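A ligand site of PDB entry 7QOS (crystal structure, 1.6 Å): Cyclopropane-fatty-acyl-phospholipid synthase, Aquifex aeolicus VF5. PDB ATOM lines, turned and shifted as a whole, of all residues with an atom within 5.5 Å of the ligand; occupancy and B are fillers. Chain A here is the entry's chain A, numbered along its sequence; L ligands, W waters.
Merely in contact with the ligand: Thr 134, Cys 175, Ile 195, Ser 198, Leu 223, Gly 242 and Met 243. Hydrophobic or aromatic side chains that line the ligand: Ile 195, Leu 197, His 224, Tyr 225, Val 241 and Met 243. Within 4 Å of the ligand: Thr 134, Tyr 135, Ser 136, Gly 174, Cys 175, Gly 176, Ile 195, Thr 196, Leu 197, Ser 198, Gln 201, Leu 223, His 224, Tyr 225, Val 241, Gly 242 and Met 243.
An oxygen (O1) of the ligand sits at hydrogen-bond distance from the side-chain hydroxyl (OG) of Ser 136 (2.6 Å). The backbone carbonyl oxygen (O) of Val 241 is in hydrogen-bond range of a nitrogen (N1) of the ligand (2.8 Å). The backbone carbonyl oxygen (O) of Gly 174 sits at hydrogen-bond distance from a nitrogen (N1) of the ligand. The backbone NH of Tyr 135 lies within hydrogen-bond range of an oxygen (O2) of the ligand (2.8 Å). An oxygen (O4) of the ligand sits at hydrogen-bond distance from the side-chain amide oxygen (OE1) of Gln 201. The backbone NH (N) of Tyr 225 is in hydrogen-bond range of a nitrogen (N5) of the ligand (3.0 Å). An oxygen (O5) of the ligand sits at hydrogen-bond distance from the backbone NH (N) of Leu 197. N of Gly 176 sits at hydrogen-bond distance from O4 of the ligand (3.1 Å). An oxygen (O4) of the ligand is in hydrogen-bond range of the side-chain hydroxyl (OG1) of Thr 196, 3.1 Å away. NE2 of His 224 lies within hydrogen-bond range of N4 of the ligand (3.4 Å).
NZ of Lys 154 is in hydrogen-bond range of OG of Ser 136 (2.8 Å). The backbone NH (N) of Gly 174 sits at hydrogen-bond distance from the backbone carbonyl oxygen (O) of Ile 195 (2.9 Å). The side-chain amide oxygen (OE1) of Gln 201 sits at hydrogen-bond distance from the side-chain hydroxyl (OG1) of Thr 196, at 2.6 Å. The backbone carbonyl oxygen (O) of Thr 196 lies within hydrogen-bond range of the backbone NH (N) of Leu 223. The side-chain hydroxyl (OG1) of Thr 196 is in hydrogen-bond range of the backbone NH (N) of Ser 198. The side-chain hydroxyl (OG) of Ser 179 sits at hydrogen-bond distance from the side-chain hydroxyl (OG1) of Thr 134 (3.1 Å). The backbone NH of Cys 175 is in hydrogen-bond range of the backbone carbonyl oxygen of Ile 195. The backbone NH of Ile 195 lies within hydrogen-bond range of the backbone carbonyl oxygen of Asp 172 (3.1 Å).
Water W1 lies within hydrogen-bond range of the backbone carbonyl oxygen (O) of Met 133 (2.7 Å), an oxygen (O2) of the ligand (2.7 Å) and the backbone NH (N) of Trp 177 (2.9 Å). Water W7 lies within hydrogen-bond range of OD2 of Asp 172 (2.7 Å) and N1 of the ligand (2.8 Å). Water W3 bridges a nitrogen (N4) of the ligand and the backbone carbonyl oxygen (O) of His 246.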
ATOM      1  N   MET A 133       2.419 -18.104 -17.131  1.00  0.00           N
ATOM      2  CA  MET A 133       3.177 -17.379 -16.104  1.00  0.00           C
ATOM      3  C   MET A 133       3.332 -15.906 -16.458  1.00  0.00           C
ATOM      4  O   MET A 133       4.372 -15.291 -16.222  1.00  0.00           O
ATOM      5  CB  MET A 133       4.541 -18.038 -15.872  1.00  0.00           C
ATOM      6  CG  MET A 133       4.451 -19.434 -15.251  1.00  0.00           C
ATOM      7  SD  MET A 133       4.087 -19.370 -13.496  1.00  0.00           S
ATOM      8  CE  MET A 133       5.680 -18.899 -12.794  1.00  0.00           C
ATOM      9  N   THR A 134       2.285 -15.340 -17.041  1.00  0.00           N
ATOM     10  CA  THR A 134       2.313 -13.928 -17.439  1.00  0.00           C
ATOM     11  C   THR A 134       1.903 -13.055 -16.256  1.00  0.00           C
ATOM     12  O   THR A 134       0.836 -13.257 -15.663  1.00  0.00           O
ATOM     13  CB  THR A 134       1.395 -13.697 -18.635  1.00  0.00           C
ATOM     14  OG1 THR A 134       1.877 -14.454 -19.762  1.00  0.00           O
ATOM     15  CG2 THR A 134       1.396 -12.229 -19.015  1.00  0.00           C
ATOM     16  N   TYR A 135       2.752 -12.088 -15.912  1.00  0.00           N
ATOM     17  CA  TYR A 135       2.559 -11.236 -14.731  1.00  0.00           C
ATOM     18  C   TYR A 135       2.328  -9.808 -15.203  1.00  0.00           C
ATOM     19  O   TYR A 135       3.199  -8.958 -15.010  1.00  0.00           O
ATOM     20  CB  TYR A 135       3.765 -11.333 -13.794  1.00  0.00           C
ATOM     21  CG  TYR A 135       3.577 -10.817 -12.390  1.00  0.00           C
ATOM     22  CD1 TYR A 135       2.310 -10.560 -11.872  1.00  0.00           C
ATOM     23  CD2 TYR A 135       4.675 -10.610 -11.568  1.00  0.00           C
ATOM     24  CE1 TYR A 135       2.153 -10.107 -10.549  1.00  0.00           C
ATOM     25  CE2 TYR A 135       4.536 -10.167 -10.267  1.00  0.00           C
ATOM     26  CZ  TYR A 135       3.281  -9.920  -9.767  1.00  0.00           C
ATOM     27  OH  TYR A 135       3.166  -9.460  -8.472  1.00  0.00           O
ATOM     28  N   SER A 136       1.163  -9.572 -15.798  1.00  0.00           N
ATOM     29  CA  SER A 136       0.795  -8.304 -16.390  1.00  0.00           C
ATOM     30  C   SER A 136      -0.660  -8.387 -16.838  1.00  0.00           C
ATOM     31  O   SER A 136      -1.274  -9.456 -16.831  1.00  0.00           O
ATOM     32  CB  SER A 136       1.720  -7.951 -17.568  1.00  0.00           C
ATOM     33  OG  SER A 136       1.758  -8.999 -18.529  1.00  0.00           O
ATOM     34  N   LYS A 154      -4.172 -11.203 -25.207  1.00  0.00           N
ATOM     35  CA  LYS A 154      -3.280 -10.069 -24.970  1.00  0.00           C
ATOM     36  C   LYS A 154      -1.991 -10.197 -25.775  1.00  0.00           C
ATOM     37  O   LYS A 154      -1.525  -9.221 -26.381  1.00  0.00           O
ATOM     38  CB  LYS A 154      -2.997  -9.957 -23.467  1.00  0.00           C
ATOM     39  CG  LYS A 154      -1.871  -9.015 -23.089  1.00  0.00           C
ATOM     40  CD  LYS A 154      -0.596  -9.852 -22.849  1.00  0.00           C
ATOM     41  CE  LYS A 154       0.361  -9.245 -21.842  1.00  0.00           C
ATOM     42  NZ  LYS A 154      -0.212  -9.330 -20.457  1.00  0.00           N
ATOM     43  N   ASP A 172      12.427  -8.195 -25.876  1.00  0.00           N
ATOM     44  CA  ASP A 172      11.458  -8.062 -24.787  1.00  0.00           C
ATOM     45  C   ASP A 172      12.195  -7.574 -23.549  1.00  0.00           C
ATOM     46  O   ASP A 172      12.987  -8.313 -22.949  1.00  0.00           O
ATOM     47  CB  ASP A 172      10.742  -9.395 -24.537  1.00  0.00           C
ATOM     48  CG  ASP A 172       9.640  -9.286 -23.491  1.00  0.00           C
ATOM     49  OD1 ASP A 172       9.581  -8.245 -22.808  1.00  0.00           O
ATOM     50  OD2 ASP A 172       8.834 -10.239 -23.349  1.00  0.00           O
ATOM     51  N   ILE A 173      11.932  -6.331 -23.163  1.00  0.00           N
ATOM     52  CA  ILE A 173      12.630  -5.696 -22.057  1.00  0.00           C
ATOM     53  C   ILE A 173      11.850  -5.977 -20.776  1.00  0.00           C
ATOM     54  O   ILE A 173      10.784  -5.389 -20.540  1.00  0.00           O
ATOM     55  CB  ILE A 173      12.801  -4.192 -22.289  1.00  0.00           C
ATOM     56  CG1 ILE A 173      13.576  -3.960 -23.598  1.00  0.00           C
ATOM     57  CG2 ILE A 173      13.519  -3.555 -21.119  1.00  0.00           C
ATOM     58  CD1 ILE A 173      13.652  -2.514 -24.006  1.00  0.00           C
ATOM     59  N   GLY A 174      12.374  -6.869 -19.935  1.00  0.00           N
ATOM     60  CA  GLY A 174      11.684  -7.297 -18.735  1.00  0.00           C
ATOM     61  C   GLY A 174      10.769  -8.468 -19.030  1.00  0.00           C
ATOM     62  O   GLY A 174       9.560  -8.378 -18.830  1.00  0.00           O
ATOM     63  N   CYS A 175      11.342  -9.583 -19.501  1.00  0.00           N
ATOM     64  CA  CYS A 175      10.566 -10.634 -20.144  1.00  0.00           C
ATOM     65  C   CYS A 175       9.876 -11.592 -19.174  1.00  0.00           C
ATOM     66  O   CYS A 175       9.128 -12.455 -19.630  1.00  0.00           O
ATOM     67  CB  CYS A 175      11.462 -11.439 -21.085  1.00  0.00           C
ATOM     68  SG  CYS A 175      12.796 -12.338 -20.226  1.00  0.00           S
ATOM     69  N   GLY A 176      10.097 -11.435 -17.880  1.00  0.00           N
ATOM     70  CA  GLY A 176       9.437 -12.305 -16.908  1.00  0.00           C
ATOM     71  C   GLY A 176       9.774 -13.752 -17.185  1.00  0.00           C
ATOM     72  O   GLY A 176      10.931 -14.098 -17.446  1.00  0.00           O
ATOM     73  N   TRP A 177       8.742 -14.601 -17.185  1.00  0.00           N
ATOM     74  CA  TRP A 177       8.891 -16.026 -17.402  1.00  0.00           C
ATOM     75  C   TRP A 177       8.822 -16.419 -18.874  1.00  0.00           C
ATOM     76  O   TRP A 177       8.637 -17.604 -19.194  1.00  0.00           O
ATOM     77  CB  TRP A 177       7.836 -16.780 -16.570  1.00  0.00           C
ATOM     78  CG  TRP A 177       8.143 -16.780 -15.091  1.00  0.00           C
ATOM     79  CD1 TRP A 177       8.992 -17.647 -14.428  1.00  0.00           C
ATOM     80  CD2 TRP A 177       7.644 -15.874 -14.084  1.00  0.00           C
ATOM     81  NE1 TRP A 177       9.039 -17.334 -13.090  1.00  0.00           N
ATOM     82  CE2 TRP A 177       8.228 -16.249 -12.850  1.00  0.00           C
ATOM     83  CE3 TRP A 177       6.756 -14.784 -14.099  1.00  0.00           C
ATOM     84  CZ2 TRP A 177       7.949 -15.582 -11.655  1.00  0.00           C
ATOM     85  CZ3 TRP A 177       6.484 -14.119 -12.910  1.00  0.00           C
ATOM     86  CH2 TRP A 177       7.071 -14.523 -11.699  1.00  0.00           C
ATOM     87  N   SER A 179       6.938 -15.839 -21.797  1.00  0.00           N
ATOM     88  CA  SER A 179       5.881 -16.269 -22.712  1.00  0.00           C
ATOM     89  C   SER A 179       5.958 -15.546 -24.062  1.00  0.00           C
ATOM     90  O   SER A 179       5.711 -16.169 -25.106  1.00  0.00           O
ATOM     91  CB  SER A 179       4.510 -16.088 -22.076  1.00  0.00           C
ATOM     92  OG  SER A 179       4.272 -14.741 -21.700  1.00  0.00           O
ATOM     93  N   ILE A 195      15.349  -9.909 -21.693  1.00  0.00           N
ATOM     94  CA  ILE A 195      16.181  -9.626 -20.529  1.00  0.00           C
ATOM     95  C   ILE A 195      15.289  -9.553 -19.295  1.00  0.00           C
ATOM     96  O   ILE A 195      14.139  -9.096 -19.356  1.00  0.00           O
ATOM     97  CB  ILE A 195      17.026  -8.348 -20.685  1.00  0.00           C
ATOM     98  CG1 ILE A 195      16.165  -7.077 -20.710  1.00  0.00           C
ATOM     99  CG2 ILE A 195      17.884  -8.407 -21.938  1.00  0.00           C
ATOM    100  CD1 ILE A 195      17.011  -5.803 -20.560  1.00  0.00           C
ATOM    101  N   THR A 196      15.805 -10.050 -18.179  1.00  0.00           N
ATOM    102  CA  THR A 196      15.131 -10.006 -16.888  1.00  0.00           C
ATOM    103  C   THR A 196      16.181  -9.765 -15.807  1.00  0.00           C
ATOM    104  O   THR A 196      17.357 -10.044 -16.003  1.00  0.00           O
ATOM    105  CB  THR A 196      14.361 -11.315 -16.615  1.00  0.00           C
ATOM    106  OG1 THR A 196      13.743 -11.260 -15.317  1.00  0.00           O
ATOM    107  CG2 THR A 196      15.302 -12.507 -16.674  1.00  0.00           C
ATOM    108  N   LEU A 197      15.736  -9.223 -14.674  1.00  0.00           N
ATOM    109  CA  LEU A 197      16.602  -9.105 -13.505  1.00  0.00           C
ATOM    110  C   LEU A 197      16.515 -10.297 -12.558  1.00  0.00           C
ATOM    111  O   LEU A 197      17.362 -10.409 -11.658  1.00  0.00           O
ATOM    112  CB  LEU A 197      16.250  -7.850 -12.699  1.00  0.00           C
ATOM    113  CG  LEU A 197      16.505  -6.515 -13.387  1.00  0.00           C
ATOM    114  CD1 LEU A 197      16.210  -5.396 -12.408  1.00  0.00           C
ATOM    115  CD2 LEU A 197      17.940  -6.459 -13.870  1.00  0.00           C
ATOM    116  N   SER A 198      15.548 -11.193 -12.737  1.00  0.00           N
ATOM    117  CA  SER A 198      15.291 -12.257 -11.770  1.00  0.00           C
ATOM    118  C   SER A 198      16.054 -13.519 -12.157  1.00  0.00           C
ATOM    119  O   SER A 198      15.894 -14.021 -13.267  1.00  0.00           O
ATOM    120  CB  SER A 198      13.788 -12.547 -11.677  1.00  0.00           C
ATOM    121  OG  SER A 198      13.526 -13.829 -11.122  1.00  0.00           O
ATOM    122  N   GLN A 201      13.495 -16.280 -12.853  1.00  0.00           N
ATOM    123  CA  GLN A 201      12.914 -16.214 -14.193  1.00  0.00           C
ATOM    124  C   GLN A 201      13.927 -16.630 -15.249  1.00  0.00           C
ATOM    125  O   GLN A 201      13.591 -17.374 -16.175  1.00  0.00           O
ATOM    126  CB  GLN A 201      12.393 -14.804 -14.475  1.00  0.00           C
ATOM    127  CG  GLN A 201      11.213 -14.411 -13.567  1.00  0.00           C
ATOM    128  CD  GLN A 201      10.817 -12.963 -13.679  1.00  0.00           C
ATOM    129  OE1 GLN A 201      11.510 -12.147 -14.304  1.00  0.00           O
ATOM    130  NE2 GLN A 201       9.700 -12.608 -13.042  1.00  0.00           N
ATOM    131  N   LEU A 223      19.907  -9.195 -17.171  1.00  0.00           N
ATOM    132  CA  LEU A 223      20.499  -7.944 -17.633  1.00  0.00           C
ATOM    133  C   LEU A 223      19.574  -6.794 -17.308  1.00  0.00           C
ATOM    134  O   LEU A 223      18.365  -6.870 -17.578  1.00  0.00           O
ATOM    135  CB  LEU A 223      20.753  -7.989 -19.141  1.00  0.00           C
ATOM    136  CG  LEU A 223      21.689  -6.891 -19.632  1.00  0.00           C
ATOM    137  CD1 LEU A 223      23.114  -7.198 -19.159  1.00  0.00           C
ATOM    138  CD2 LEU A 223      21.629  -6.759 -21.145  1.00  0.00           C
ATOM    139  N   HIS A 224      20.154  -5.733 -16.738  1.00  0.00           N
ATOM    140  CA  HIS A 224      19.492  -4.445 -16.586  1.00  0.00           C
ATOM    141  C   HIS A 224      19.385  -3.751 -17.945  1.00  0.00           C
ATOM    142  O   HIS A 224      20.303  -3.841 -18.764  1.00  0.00           O
ATOM    143  CB  HIS A 224      20.316  -3.603 -15.602  1.00  0.00           C
ATOM    144  CG  HIS A 224      19.619  -2.392 -15.053  1.00  0.00           C
ATOM    145  ND1 HIS A 224      19.386  -1.263 -15.805  1.00  0.00           N
ATOM    146  CD2 HIS A 224      19.187  -2.114 -13.795  1.00  0.00           C
ATOM    147  CE1 HIS A 224      18.801  -0.351 -15.047  1.00  0.00           C
ATOM    148  NE2 HIS A 224      18.677  -0.839 -13.830  1.00  0.00           N
ATOM    149  N   TYR A 225      18.267  -3.046 -18.188  1.00  0.00           N
ATOM    150  CA  TYR A 225      18.054  -2.440 -19.499  1.00  0.00           C
ATOM    151  C   TYR A 225      19.175  -1.451 -19.853  1.00  0.00           C
ATOM    152  O   TYR A 225      19.476  -1.265 -21.035  1.00  0.00           O
ATOM    153  CB  TYR A 225      16.698  -1.726 -19.574  1.00  0.00           C
ATOM    154  CG  TYR A 225      16.656  -0.438 -18.773  1.00  0.00           C
ATOM    155  CD1 TYR A 225      17.097   0.758 -19.313  1.00  0.00           C
ATOM    156  CD2 TYR A 225      16.174  -0.432 -17.478  1.00  0.00           C
ATOM    157  CE1 TYR A 225      17.083   1.926 -18.565  1.00  0.00           C
ATOM    158  CE2 TYR A 225      16.146   0.732 -16.729  1.00  0.00           C
ATOM    159  CZ  TYR A 225      16.598   1.897 -17.282  1.00  0.00           C
ATOM    160  OH  TYR A 225      16.581   3.051 -16.533  1.00  0.00           O
ATOM    161  N   VAL A 241       6.449  -4.991 -21.265  1.00  0.00           N
ATOM    162  CA  VAL A 241       5.133  -5.166 -20.648  1.00  0.00           C
ATOM    163  C   VAL A 241       5.325  -5.331 -19.150  1.00  0.00           C
ATOM    164  O   VAL A 241       5.926  -6.312 -18.706  1.00  0.00           O
ATOM    165  CB  VAL A 241       4.406  -6.385 -21.228  1.00  0.00           C
ATOM    166  CG1 VAL A 241       3.048  -6.596 -20.555  1.00  0.00           C
ATOM    167  CG2 VAL A 241       4.238  -6.247 -22.738  1.00  0.00           C
ATOM    168  N   GLY A 242       4.777  -4.397 -18.362  1.00  0.00           N
ATOM    169  CA  GLY A 242       4.823  -4.547 -16.919  1.00  0.00           C
ATOM    170  C   GLY A 242       6.203  -4.386 -16.316  1.00  0.00           C
ATOM    171  O   GLY A 242       6.418  -4.788 -15.166  1.00  0.00           O
ATOM    172  N   MET A 243       7.143  -3.804 -17.053  1.00  0.00           N
ATOM    173  CA  MET A 243       8.484  -3.540 -16.554  1.00  0.00           C
ATOM    174  C   MET A 243       8.694  -2.057 -16.243  1.00  0.00           C
ATOM    175  O   MET A 243       9.388  -1.730 -15.272  1.00  0.00           O
ATOM    176  CB  MET A 243       9.514  -4.032 -17.582  1.00  0.00           C
ATOM    177  CG  MET A 243      10.954  -3.626 -17.316  1.00  0.00           C
ATOM    178  SD  MET A 243      11.306  -2.063 -18.156  1.00  0.00           S
ATOM    179  CE  MET A 243      12.998  -1.847 -17.598  1.00  0.00           C
ATOM    180  N   HIS A 246       8.844  -0.206 -12.840  1.00  0.00           N
ATOM    181  CA  HIS A 246       9.991  -0.384 -11.968  1.00  0.00           C
ATOM    182  C   HIS A 246      11.189   0.467 -12.368  1.00  0.00           C
ATOM    183  O   HIS A 246      12.234   0.405 -11.711  1.00  0.00           O
ATOM    184  CB  HIS A 246      10.356  -1.869 -11.926  1.00  0.00           C
ATOM    185  CG  HIS A 246       9.189  -2.726 -11.514  1.00  0.00           C
ATOM    186  ND1 HIS A 246       8.544  -3.576 -12.378  1.00  0.00           N
ATOM    187  CD2 HIS A 246       8.522  -2.805 -10.339  1.00  0.00           C
ATOM    188  CE1 HIS A 246       7.544  -4.173 -11.740  1.00  0.00           C
ATOM    189  NE2 HIS A 246       7.517  -3.722 -10.496  1.00  0.00           N
ATOM    190  N   VAL A 247      11.041   1.302 -13.398  1.00  0.00           N
ATOM    191  CA  VAL A 247      12.169   2.081 -13.898  1.00  0.00           C
ATOM    192  C   VAL A 247      12.454   3.282 -12.993  1.00  0.00           C
ATOM    193  O   VAL A 247      13.608   3.578 -12.683  1.00  0.00           O
ATOM    194  CB  VAL A 247      11.913   2.496 -15.362  1.00  0.00           C
ATOM    195  CG1 VAL A 247      12.881   3.587 -15.805  1.00  0.00           C
ATOM    196  CG2 VAL A 247      12.032   1.273 -16.264  1.00  0.00           C
HETATM  197  N1  LIG L   1       6.864  -8.860 -19.256  1.00  0.00           N
HETATM  198  C1  LIG L   1       6.571  -9.988 -18.377  1.00  0.00           C
HETATM  199  C2  LIG L   1       7.082  -9.724 -16.960  1.00  0.00           C
HETATM  200  C3  LIG L   1       6.638  -8.457 -16.237  1.00  0.00           C
HETATM  201  S1  LIG L   1       7.237  -8.539 -14.527  1.00  0.00           S
HETATM  202  C4  LIG L   1       5.086 -10.281 -18.347  1.00  0.00           C
HETATM  203  O1  LIG L   1       4.282  -9.511 -18.884  1.00  0.00           O
HETATM  204  O2  LIG L   1       4.659 -11.299 -17.817  1.00  0.00           O
HETATM  205  C5  LIG L   1       8.527  -7.268 -14.731  1.00  0.00           C
HETATM  206  C6  LIG L   1       9.766  -7.732 -15.482  1.00  0.00           C
HETATM  207  O3  LIG L   1      10.619  -6.629 -15.703  1.00  0.00           O
HETATM  208  C7  LIG L   1      10.596  -8.748 -14.717  1.00  0.00           C
HETATM  209  O4  LIG L   1      11.188  -9.601 -15.693  1.00  0.00           O
HETATM  210  C8  LIG L   1      11.692  -7.912 -14.103  1.00  0.00           C
HETATM  211  O5  LIG L   1      12.865  -8.649 -13.841  1.00  0.00           O
HETATM  212  C9  LIG L   1      11.918  -6.918 -15.221  1.00  0.00           C
HETATM  213  N2  LIG L   1      12.657  -5.699 -14.820  1.00  0.00           N
HETATM  214  C10 LIG L   1      12.422  -4.823 -13.795  1.00  0.00           C
HETATM  215  N3  LIG L   1      13.361  -3.854 -13.819  1.00  0.00           N
HETATM  216  C11 LIG L   1      14.204  -4.099 -14.866  1.00  0.00           C
HETATM  217  C12 LIG L   1      15.337  -3.465 -15.356  1.00  0.00           C
HETATM  218  N4  LIG L   1      15.807  -2.368 -14.776  1.00  0.00           N
HETATM  219  N5  LIG L   1      15.970  -3.994 -16.450  1.00  0.00           N
HETATM  220  C13 LIG L   1      15.519  -5.144 -17.058  1.00  0.00           C
HETATM  221  N6  LIG L   1      14.386  -5.778 -16.568  1.00  0.00           N
HETATM  222  C14 LIG L   1      13.766  -5.267 -15.485  1.00  0.00           C
HETATM  223  O   HOH W   1       6.070 -13.535 -17.337  1.00  0.00           O
HETATM  224  O   HOH W   2      13.876  -3.034 -10.873  1.00  0.00           O
HETATM  225  O   HOH W   3      14.896  -0.763 -12.524  1.00  0.00           O
HETATM  226  O   HOH W   4       3.783 -10.244 -21.546  1.00  0.00           O
HETATM  227  O   HOH W   5       8.217  -7.027 -21.036  1.00  0.00           O
HETATM  228  O   HOH W   6      12.659  -8.896 -11.099  1.00  0.00           O
HETATM  229  O   HOH W   7       6.644 -10.132 -21.795  1.00  0.00           O
